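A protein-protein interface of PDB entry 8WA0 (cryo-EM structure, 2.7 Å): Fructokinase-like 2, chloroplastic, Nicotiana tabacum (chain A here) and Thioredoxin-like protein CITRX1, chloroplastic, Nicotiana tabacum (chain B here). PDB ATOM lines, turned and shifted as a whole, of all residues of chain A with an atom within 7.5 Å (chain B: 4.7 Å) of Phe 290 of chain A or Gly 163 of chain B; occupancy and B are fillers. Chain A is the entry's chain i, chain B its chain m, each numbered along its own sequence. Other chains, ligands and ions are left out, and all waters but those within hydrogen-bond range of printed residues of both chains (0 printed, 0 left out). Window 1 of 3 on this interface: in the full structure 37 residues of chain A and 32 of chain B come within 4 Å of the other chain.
Among the printed residues, merely in contact across the chains: His 288 of chain A with Gly 163 of chain B, Ala 289 of chain A with Pro 145 of chain B, Phe 290 of chain A with Gly 143 of chain B, Phe 290 of chain A with Pro 145 of chain B, Phe 290 of chain A with Glu 162 of chain B, Phe 290 of chain A with Gly 163 of chain B, Val 291 of chain A with Gly 143 of chain B, Val 291 of chain A with Pro 145 of chain B, Pro 292 of chain A with Arg 142 of chain B, Phe 352 of chain A with Leu 164 of chain B, Ala 379 of chain A with Thr 161 of chain B, Phe 425 of chain A with Glu 162 of chain B and Pro 457 of chain A with Arg 142 of chain B.
Phe 290 of chain A touches just these residues of chain B: Gly 143 (3.3 Å), Pro 145 (3.9 Å), Glu 162 (3.3 Å) and Gly 163 (3.6 Å).
Gly 163 of chain B touches just these residues of chain A: His 288 (3.6 Å) and Phe 290 (3.6 Å).
Of the printed residues of chain A, Arg 142 of chain B touches Pro 292 and Pro 457.
Printed residues of chain A within 4 Å of Thr 161 of chain B: Ala 379 (3.4 Å).
The nearest residue of chain A that does not touch Gly 163 of chain B is Ala 289 of chain A (4.1 Å).
The nearest printed residue of chain A that does not touch Pro 145 of chain B is His 288 of chain A (6.0 Å).
O of His 288 of chain A is in hydrogen-bond range of N of Leu 164 of chain B (3.2 Å).
The backbone carbonyl oxygen (O) of Ala 379 of chain A lies within hydrogen-bond range of the backbone NH (N) of Glu 162 of chain B, at 3.5 Å.
Of the 10 printed residues of chain B, 7 touch a printed residue of chain A.
Printed residues of chain B that touch a printed residue of chain A: Arg 142, Gly 143, Pro 145, Thr 161, Glu 162, Gly 163 and Leu 164.
Hydrophobic or aromatic side chains of chain B within 4 Å of the printed part of chain A: Pro 145 and Leu 164.
Printed residues of chain A that touch a printed residue of chain B: His 288, Ala 289, Phe 290, Val 291, Pro 292, Phe 352, Ala 379, Phe 425 and Pro 457.
Hydrophobic or aromatic side chains of chain A that line the printed part of chain B: His 288, Phe 290, Phe 352, Ala 379, Phe 425 and Pro 457.
Along chain A the printed residues that touch a printed residue of chain B span positions 288 to 457.
Among the printed residues, no Asp or Glu carboxylate lies within 4 Å of a Lys or Arg side-chain nitrogen of the other chain.
The side-chain carboxylate (OE2) of Glu 162 of chain B lies within salt-bridge range of the guanidinium group (NE) of Arg 142 of chain B, at 2.9 Å.
OG1 of Thr 146 of chain B is in hydrogen-bond range of O of Gly 143 of chain B, 3.1 Å away.
N of Gly 163 of chain B lies within hydrogen-bond range of O of Pro 145 of chain B.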
ATOM      1  N   ALA A 286     -23.871  20.993 -18.237  1.00  0.00           N
ATOM      2  CA  ALA A 286     -24.276  21.061 -16.851  1.00  0.00           C
ATOM      3  C   ALA A 286     -25.638  20.450 -16.749  1.00  0.00           C
ATOM      4  O   ALA A 286     -26.559  20.877 -17.427  1.00  0.00           O
ATOM      5  CB  ALA A 286     -24.333  22.488 -16.386  1.00  0.00           C
ATOM      6  N   GLN A 287     -25.780  19.451 -15.899  1.00  0.00           N
ATOM      7  CA  GLN A 287     -27.047  18.778 -15.740  1.00  0.00           C
ATOM      8  C   GLN A 287     -27.243  18.474 -14.283  1.00  0.00           C
ATOM      9  O   GLN A 287     -26.289  18.460 -13.525  1.00  0.00           O
ATOM     10  CB  GLN A 287     -27.046  17.486 -16.541  1.00  0.00           C
ATOM     11  CG  GLN A 287     -27.342  17.661 -18.018  1.00  0.00           C
ATOM     12  CD  GLN A 287     -26.511  16.739 -18.880  1.00  0.00           C
ATOM     13  OE1 GLN A 287     -26.740  16.624 -20.082  1.00  0.00           O
ATOM     14  NE2 GLN A 287     -25.538  16.077 -18.270  1.00  0.00           N
ATOM     15  N   HIS A 288     -28.476  18.240 -13.878  1.00  0.00           N
ATOM     16  CA  HIS A 288     -28.752  17.892 -12.502  1.00  0.00           C
ATOM     17  C   HIS A 288     -29.130  16.443 -12.485  1.00  0.00           C
ATOM     18  O   HIS A 288     -30.047  16.046 -13.188  1.00  0.00           O
ATOM     19  CB  HIS A 288     -29.915  18.734 -11.999  1.00  0.00           C
ATOM     20  CG  HIS A 288     -30.297  18.482 -10.578  1.00  0.00           C
ATOM     21  ND1 HIS A 288     -29.595  19.003  -9.514  1.00  0.00           N
ATOM     22  CD2 HIS A 288     -31.336  17.799 -10.044  1.00  0.00           C
ATOM     23  CE1 HIS A 288     -30.170  18.632  -8.385  1.00  0.00           C
ATOM     24  NE2 HIS A 288     -31.230  17.900  -8.679  1.00  0.00           N
ATOM     25  N   ALA A 289     -28.387  15.633 -11.750  1.00  0.00           N
ATOM     26  CA  ALA A 289     -28.689  14.214 -11.625  1.00  0.00           C
ATOM     27  C   ALA A 289     -28.878  13.468 -12.927  1.00  0.00           C
ATOM     28  O   ALA A 289     -29.971  13.021 -13.230  1.00  0.00           O
ATOM     29  CB  ALA A 289     -29.902  14.023 -10.741  1.00  0.00           C
ATOM     30  N   PHE A 290     -27.811  13.303 -13.687  1.00  0.00           N
ATOM     31  CA  PHE A 290     -27.905  12.581 -14.936  1.00  0.00           C
ATOM     32  C   PHE A 290     -26.958  11.418 -14.935  1.00  0.00           C
ATOM     33  O   PHE A 290     -25.796  11.572 -14.603  1.00  0.00           O
ATOM     34  CB  PHE A 290     -27.547  13.503 -16.076  1.00  0.00           C
ATOM     35  CG  PHE A 290     -28.084  13.061 -17.394  1.00  0.00           C
ATOM     36  CD1 PHE A 290     -29.441  13.073 -17.630  1.00  0.00           C
ATOM     37  CD2 PHE A 290     -27.234  12.646 -18.395  1.00  0.00           C
ATOM     38  CE1 PHE A 290     -29.948  12.668 -18.843  1.00  0.00           C
ATOM     39  CE2 PHE A 290     -27.734  12.243 -19.609  1.00  0.00           C
ATOM     40  CZ  PHE A 290     -29.092  12.265 -19.836  1.00  0.00           C
ATOM     41  N   VAL A 291     -27.443  10.249 -15.310  1.00  0.00           N
ATOM     42  CA  VAL A 291     -26.604   9.068 -15.311  1.00  0.00           C
ATOM     43  C   VAL A 291     -26.395   8.571 -16.725  1.00  0.00           C
ATOM     44  O   VAL A 291     -27.348   8.214 -17.400  1.00  0.00           O
ATOM     45  CB  VAL A 291     -27.265   7.941 -14.511  1.00  0.00           C
ATOM     46  CG1 VAL A 291     -26.336   6.751 -14.413  1.00  0.00           C
ATOM     47  CG2 VAL A 291     -27.646   8.425 -13.123  1.00  0.00           C
ATOM     48  N   PRO A 292     -25.144   8.531 -17.179  1.00  0.00           N
ATOM     49  CA  PRO A 292     -24.897   8.132 -18.557  1.00  0.00           C
ATOM     50  C   PRO A 292     -25.275   6.711 -18.879  1.00  0.00           C
ATOM     51  O   PRO A 292     -25.914   6.486 -19.892  1.00  0.00           O
ATOM     52  CB  PRO A 292     -23.393   8.252 -18.668  1.00  0.00           C
ATOM     53  CG  PRO A 292     -23.007   9.266 -17.654  1.00  0.00           C
ATOM     54  CD  PRO A 292     -23.927   9.006 -16.509  1.00  0.00           C
ATOM     55  N   SER A 293     -24.917   5.763 -18.031  1.00  0.00           N
ATOM     56  CA  SER A 293     -25.169   4.353 -18.312  1.00  0.00           C
ATOM     57  C   SER A 293     -25.104   3.552 -17.037  1.00  0.00           C
ATOM     58  O   SER A 293     -24.781   4.094 -15.997  1.00  0.00           O
ATOM     59  CB  SER A 293     -24.163   3.800 -19.298  1.00  0.00           C
ATOM     60  OG  SER A 293     -22.852   3.880 -18.793  1.00  0.00           O
ATOM     61  N   ALA A 322     -23.051   3.074 -11.996  1.00  0.00           N
ATOM     62  CA  ALA A 322     -22.876   4.114 -12.963  1.00  0.00           C
ATOM     63  C   ALA A 322     -21.450   4.440 -13.122  1.00  0.00           C
ATOM     64  O   ALA A 322     -20.697   4.408 -12.162  1.00  0.00           O
ATOM     65  CB  ALA A 322     -23.548   5.335 -12.479  1.00  0.00           C
ATOM     66  N   GLY A 324     -20.147   7.386 -13.774  1.00  0.00           N
ATOM     67  CA  GLY A 324     -19.777   8.634 -13.176  1.00  0.00           C
ATOM     68  C   GLY A 324     -20.885   9.583 -13.458  1.00  0.00           C
ATOM     69  O   GLY A 324     -21.975   9.149 -13.787  1.00  0.00           O
ATOM     70  N   GLY A 325     -20.642  10.872 -13.319  1.00  0.00           N
ATOM     71  CA  GLY A 325     -21.643  11.864 -13.619  1.00  0.00           C
ATOM     72  C   GLY A 325     -21.234  12.944 -14.579  1.00  0.00           C
ATOM     73  O   GLY A 325     -20.203  12.819 -15.223  1.00  0.00           O
ATOM     74  N   CYS A 326     -22.028  13.998 -14.699  1.00  0.00           N
ATOM     75  CA  CYS A 326     -21.729  15.131 -15.571  1.00  0.00           C
ATOM     76  C   CYS A 326     -20.550  15.987 -15.142  1.00  0.00           C
ATOM     77  O   CYS A 326     -20.158  15.949 -13.990  1.00  0.00           O
ATOM     78  CB  CYS A 326     -22.954  16.005 -15.614  1.00  0.00           C
ATOM     79  SG  CYS A 326     -23.225  17.033 -14.167  1.00  0.00           S
ATOM     80  N   ASN A 329     -20.443  18.083 -11.964  1.00  0.00           N
ATOM     81  CA  ASN A 329     -20.207  17.311 -10.750  1.00  0.00           C
ATOM     82  C   ASN A 329     -18.737  17.085 -10.451  1.00  0.00           C
ATOM     83  O   ASN A 329     -18.338  17.175  -9.305  1.00  0.00           O
ATOM     84  CB  ASN A 329     -21.007  16.037 -10.786  1.00  0.00           C
ATOM     85  CG  ASN A 329     -22.488  16.290 -10.717  1.00  0.00           C
ATOM     86  OD1 ASN A 329     -22.922  17.417 -10.511  1.00  0.00           O
ATOM     87  ND2 ASN A 329     -23.276  15.243 -10.890  1.00  0.00           N
ATOM     88  N   PHE A 352     -33.929  27.531 -14.629  1.00  0.00           N
ATOM     89  CA  PHE A 352     -33.093  26.422 -14.279  1.00  0.00           C
ATOM     90  C   PHE A 352     -31.689  26.823 -14.492  1.00  0.00           C
ATOM     91  O   PHE A 352     -30.825  26.489 -13.693  1.00  0.00           O
ATOM     92  CB  PHE A 352     -33.392  25.163 -15.068  1.00  0.00           C
ATOM     93  CG  PHE A 352     -33.057  23.898 -14.349  1.00  0.00           C
ATOM     94  CD1 PHE A 352     -33.030  23.852 -12.971  1.00  0.00           C
ATOM     95  CD2 PHE A 352     -32.803  22.745 -15.055  1.00  0.00           C
ATOM     96  CE1 PHE A 352     -32.729  22.680 -12.312  1.00  0.00           C
ATOM     97  CE2 PHE A 352     -32.502  21.573 -14.409  1.00  0.00           C
ATOM     98  CZ  PHE A 352     -32.467  21.537 -13.035  1.00  0.00           C
ATOM     99  N   ALA A 379     -32.968  22.313 -20.634  1.00  0.00           N
ATOM    100  CA  ALA A 379     -32.835  20.882 -20.832  1.00  0.00           C
ATOM    101  C   ALA A 379     -33.774  20.339 -21.871  1.00  0.00           C
ATOM    102  O   ALA A 379     -33.911  19.132 -21.982  1.00  0.00           O
ATOM    103  CB  ALA A 379     -33.034  20.166 -19.528  1.00  0.00           C
ATOM    104  N   PHE A 425     -19.890  12.466 -23.741  1.00  0.00           N
ATOM    105  CA  PHE A 425     -21.196  13.012 -23.952  1.00  0.00           C
ATOM    106  C   PHE A 425     -21.211  14.245 -24.810  1.00  0.00           C
ATOM    107  O   PHE A 425     -22.111  14.406 -25.614  1.00  0.00           O
ATOM    108  CB  PHE A 425     -21.732  13.409 -22.620  1.00  0.00           C
ATOM    109  CG  PHE A 425     -23.217  13.422 -22.520  1.00  0.00           C
ATOM    110  CD1 PHE A 425     -23.921  12.243 -22.420  1.00  0.00           C
ATOM    111  CD2 PHE A 425     -23.899  14.615 -22.444  1.00  0.00           C
ATOM    112  CE1 PHE A 425     -25.282  12.255 -22.289  1.00  0.00           C
ATOM    113  CE2 PHE A 425     -25.258  14.636 -22.312  1.00  0.00           C
ATOM    114  CZ  PHE A 425     -25.949  13.453 -22.227  1.00  0.00           C
ATOM    115  N   PRO A 457     -22.151   6.654 -23.101  1.00  0.00           N
ATOM    116  CA  PRO A 457     -23.567   6.756 -22.776  1.00  0.00           C
ATOM    117  C   PRO A 457     -24.389   5.602 -23.292  1.00  0.00           C
ATOM    118  O   PRO A 457     -23.847   4.717 -23.925  1.00  0.00           O
ATOM    119  CB  PRO A 457     -23.989   8.048 -23.466  1.00  0.00           C
ATOM    120  CG  PRO A 457     -22.731   8.790 -23.734  1.00  0.00           C
ATOM    121  CD  PRO A 457     -21.792   7.695 -24.090  1.00  0.00           C
ATOM    122  N   SER A 565     -22.847   6.794  -8.391  1.00  0.00           N
ATOM    123  CA  SER A 565     -22.316   7.857  -9.220  1.00  0.00           C
ATOM    124  C   SER A 565     -21.378   8.761  -8.485  1.00  0.00           C
ATOM    125  O   SER A 565     -20.383   9.189  -9.047  1.00  0.00           O
ATOM    126  CB  SER A 565     -23.449   8.717  -9.737  1.00  0.00           C
ATOM    127  OG  SER A 565     -24.360   7.960 -10.504  1.00  0.00           O
ATOM    128  N   ASP A 569     -17.287  10.563  -9.428  1.00  0.00           N
ATOM    129  CA  ASP A 569     -16.859  11.952  -9.473  1.00  0.00           C
ATOM    130  C   ASP A 569     -15.765  12.254  -8.497  1.00  0.00           C
ATOM    131  O   ASP A 569     -14.858  13.005  -8.816  1.00  0.00           O
ATOM    132  CB  ASP A 569     -18.031  12.831  -9.214  1.00  0.00           C
ATOM    133  CG  ASP A 569     -19.214  12.489 -10.086  1.00  0.00           C
ATOM    134  OD1 ASP A 569     -19.000  12.065 -11.240  1.00  0.00           O
ATOM    135  OD2 ASP A 569     -20.363  12.647  -9.620  1.00  0.00           O
ATOM    136  N   MET B 107     -37.591  10.889  -9.288  1.00  0.00           N
ATOM    137  CA  MET B 107     -38.405  11.395 -10.384  1.00  0.00           C
ATOM    138  C   MET B 107     -39.784  10.800 -10.355  1.00  0.00           C
ATOM    139  O   MET B 107     -40.766  11.489 -10.599  1.00  0.00           O
ATOM    140  CB  MET B 107     -37.753  11.073 -11.718  1.00  0.00           C
ATOM    141  CG  MET B 107     -38.560  11.470 -12.938  1.00  0.00           C
ATOM    142  SD  MET B 107     -38.481  13.236 -13.260  1.00  0.00           S
ATOM    143  CE  MET B 107     -36.936  13.342 -14.154  1.00  0.00           C
ATOM    144  N   ARG B 142     -30.614   9.129 -24.201  1.00  0.00           N
ATOM    145  CA  ARG B 142     -29.188   9.328 -24.045  1.00  0.00           C
ATOM    146  C   ARG B 142     -28.731   8.964 -22.648  1.00  0.00           C
ATOM    147  O   ARG B 142     -27.673   8.375 -22.475  1.00  0.00           O
ATOM    148  CB  ARG B 142     -28.815  10.760 -24.392  1.00  0.00           C
ATOM    149  CG  ARG B 142     -29.026  11.097 -25.856  1.00  0.00           C
ATOM    150  CD  ARG B 142     -28.208  12.306 -26.269  1.00  0.00           C
ATOM    151  NE  ARG B 142     -28.516  13.478 -25.463  1.00  0.00           N
ATOM    152  CZ  ARG B 142     -27.936  14.661 -25.621  1.00  0.00           C
ATOM    153  NH1 ARG B 142     -27.013  14.826 -26.557  1.00  0.00           N
ATOM    154  NH2 ARG B 142     -28.275  15.679 -24.843  1.00  0.00           N
ATOM    155  N   GLY B 143     -29.533   9.288 -21.649  1.00  0.00           N
ATOM    156  CA  GLY B 143     -29.179   9.008 -20.274  1.00  0.00           C
ATOM    157  C   GLY B 143     -30.400   8.525 -19.558  1.00  0.00           C
ATOM    158  O   GLY B 143     -31.502   8.707 -20.047  1.00  0.00           O
ATOM    159  N   PRO B 145     -32.350   9.293 -16.645  1.00  0.00           N
ATOM    160  CA  PRO B 145     -33.577  10.007 -16.255  1.00  0.00           C
ATOM    161  C   PRO B 145     -34.157  10.853 -17.400  1.00  0.00           C
ATOM    162  O   PRO B 145     -33.998  12.067 -17.364  1.00  0.00           O
ATOM    163  CB  PRO B 145     -33.124  10.891 -15.092  1.00  0.00           C
ATOM    164  CG  PRO B 145     -31.715  10.492 -14.787  1.00  0.00           C
ATOM    165  CD  PRO B 145     -31.157   9.898 -16.038  1.00  0.00           C
ATOM    166  N   THR B 146     -34.829  10.241 -18.380  1.00  0.00           N
ATOM    167  CA  THR B 146     -35.354  10.970 -19.555  1.00  0.00           C
ATOM    168  C   THR B 146     -36.869  10.989 -19.725  1.00  0.00           C
ATOM    169  O   THR B 146     -37.512   9.947 -19.641  1.00  0.00           O
ATOM    170  CB  THR B 146     -34.771  10.422 -20.868  1.00  0.00           C
ATOM    171  OG1 THR B 146     -34.472   9.033 -20.709  1.00  0.00           O
ATOM    172  CG2 THR B 146     -33.507  11.157 -21.242  1.00  0.00           C
ATOM    173  N   THR B 161     -36.789  15.962 -22.256  1.00  0.00           N
ATOM    174  CA  THR B 161     -36.106  16.632 -21.171  1.00  0.00           C
ATOM    175  C   THR B 161     -35.165  15.645 -20.555  1.00  0.00           C
ATOM    176  O   THR B 161     -35.537  14.508 -20.316  1.00  0.00           O
ATOM    177  CB  THR B 161     -37.063  17.122 -20.108  1.00  0.00           C
ATOM    178  OG1 THR B 161     -37.351  16.055 -19.199  1.00  0.00           O
ATOM    179  CG2 THR B 161     -38.355  17.587 -20.728  1.00  0.00           C
ATOM    180  N   GLU B 162     -33.931  16.058 -20.314  1.00  0.00           N
ATOM    181  CA  GLU B 162     -32.932  15.194 -19.717  1.00  0.00           C
ATOM    182  C   GLU B 162     -32.513  15.683 -18.325  1.00  0.00           C
ATOM    183  O   GLU B 162     -32.192  16.848 -18.163  1.00  0.00           O
ATOM    184  CB  GLU B 162     -31.746  15.108 -20.644  1.00  0.00           C
ATOM    185  CG  GLU B 162     -32.067  14.505 -21.993  1.00  0.00           C
ATOM    186  CD  GLU B 162     -30.825  14.142 -22.767  1.00  0.00           C
ATOM    187  OE1 GLU B 162     -29.717  14.447 -22.285  1.00  0.00           O
ATOM    188  OE2 GLU B 162     -30.960  13.550 -23.856  1.00  0.00           O
ATOM    189  N   GLY B 163     -32.519  14.816 -17.322  1.00  0.00           N
ATOM    190  CA  GLY B 163     -32.162  15.195 -15.968  1.00  0.00           C
ATOM    191  C   GLY B 163     -33.342  15.506 -15.095  1.00  0.00           C
ATOM    192  O   GLY B 163     -34.435  15.697 -15.606  1.00  0.00           O
ATOM    193  N   LEU B 164     -33.163  15.538 -13.792  1.00  0.00           N
ATOM    194  CA  LEU B 164     -34.237  15.910 -12.911  1.00  0.00           C
ATOM    195  C   LEU B 164     -34.546  17.342 -13.172  1.00  0.00           C
ATOM    196  O   LEU B 164     -33.649  18.169 -13.181  1.00  0.00           O
ATOM    197  CB  LEU B 164     -33.825  15.729 -11.464  1.00  0.00           C
ATOM    198  CG  LEU B 164     -34.561  14.719 -10.598  1.00  0.00           C
ATOM    199  CD1 LEU B 164     -34.415  13.322 -11.176  1.00  0.00           C
ATOM    200  CD2 LEU B 164     -34.010  14.778  -9.188  1.00  0.00           C
ATOM    201  N   ILE B 165     -35.809  17.671 -13.337  1.00  0.00           N
ATOM    202  CA  ILE B 165     -36.207  19.001 -13.668  1.00  0.00           C
ATOM    203  C   ILE B 165     -37.237  19.400 -12.683  1.00  0.00           C
ATOM    204  O   ILE B 165     -37.983  18.568 -12.219  1.00  0.00           O
ATOM    205  CB  ILE B 165     -36.814  18.991 -15.051  1.00  0.00           C
ATOM    206  CG1 ILE B 165     -37.671  17.748 -15.265  1.00  0.00           C
ATOM    207  CG2 ILE B 165     -35.728  19.039 -16.112  1.00  0.00           C
ATOM    208  CD1 ILE B 165     -38.561  17.834 -16.483  1.00  0.00           C
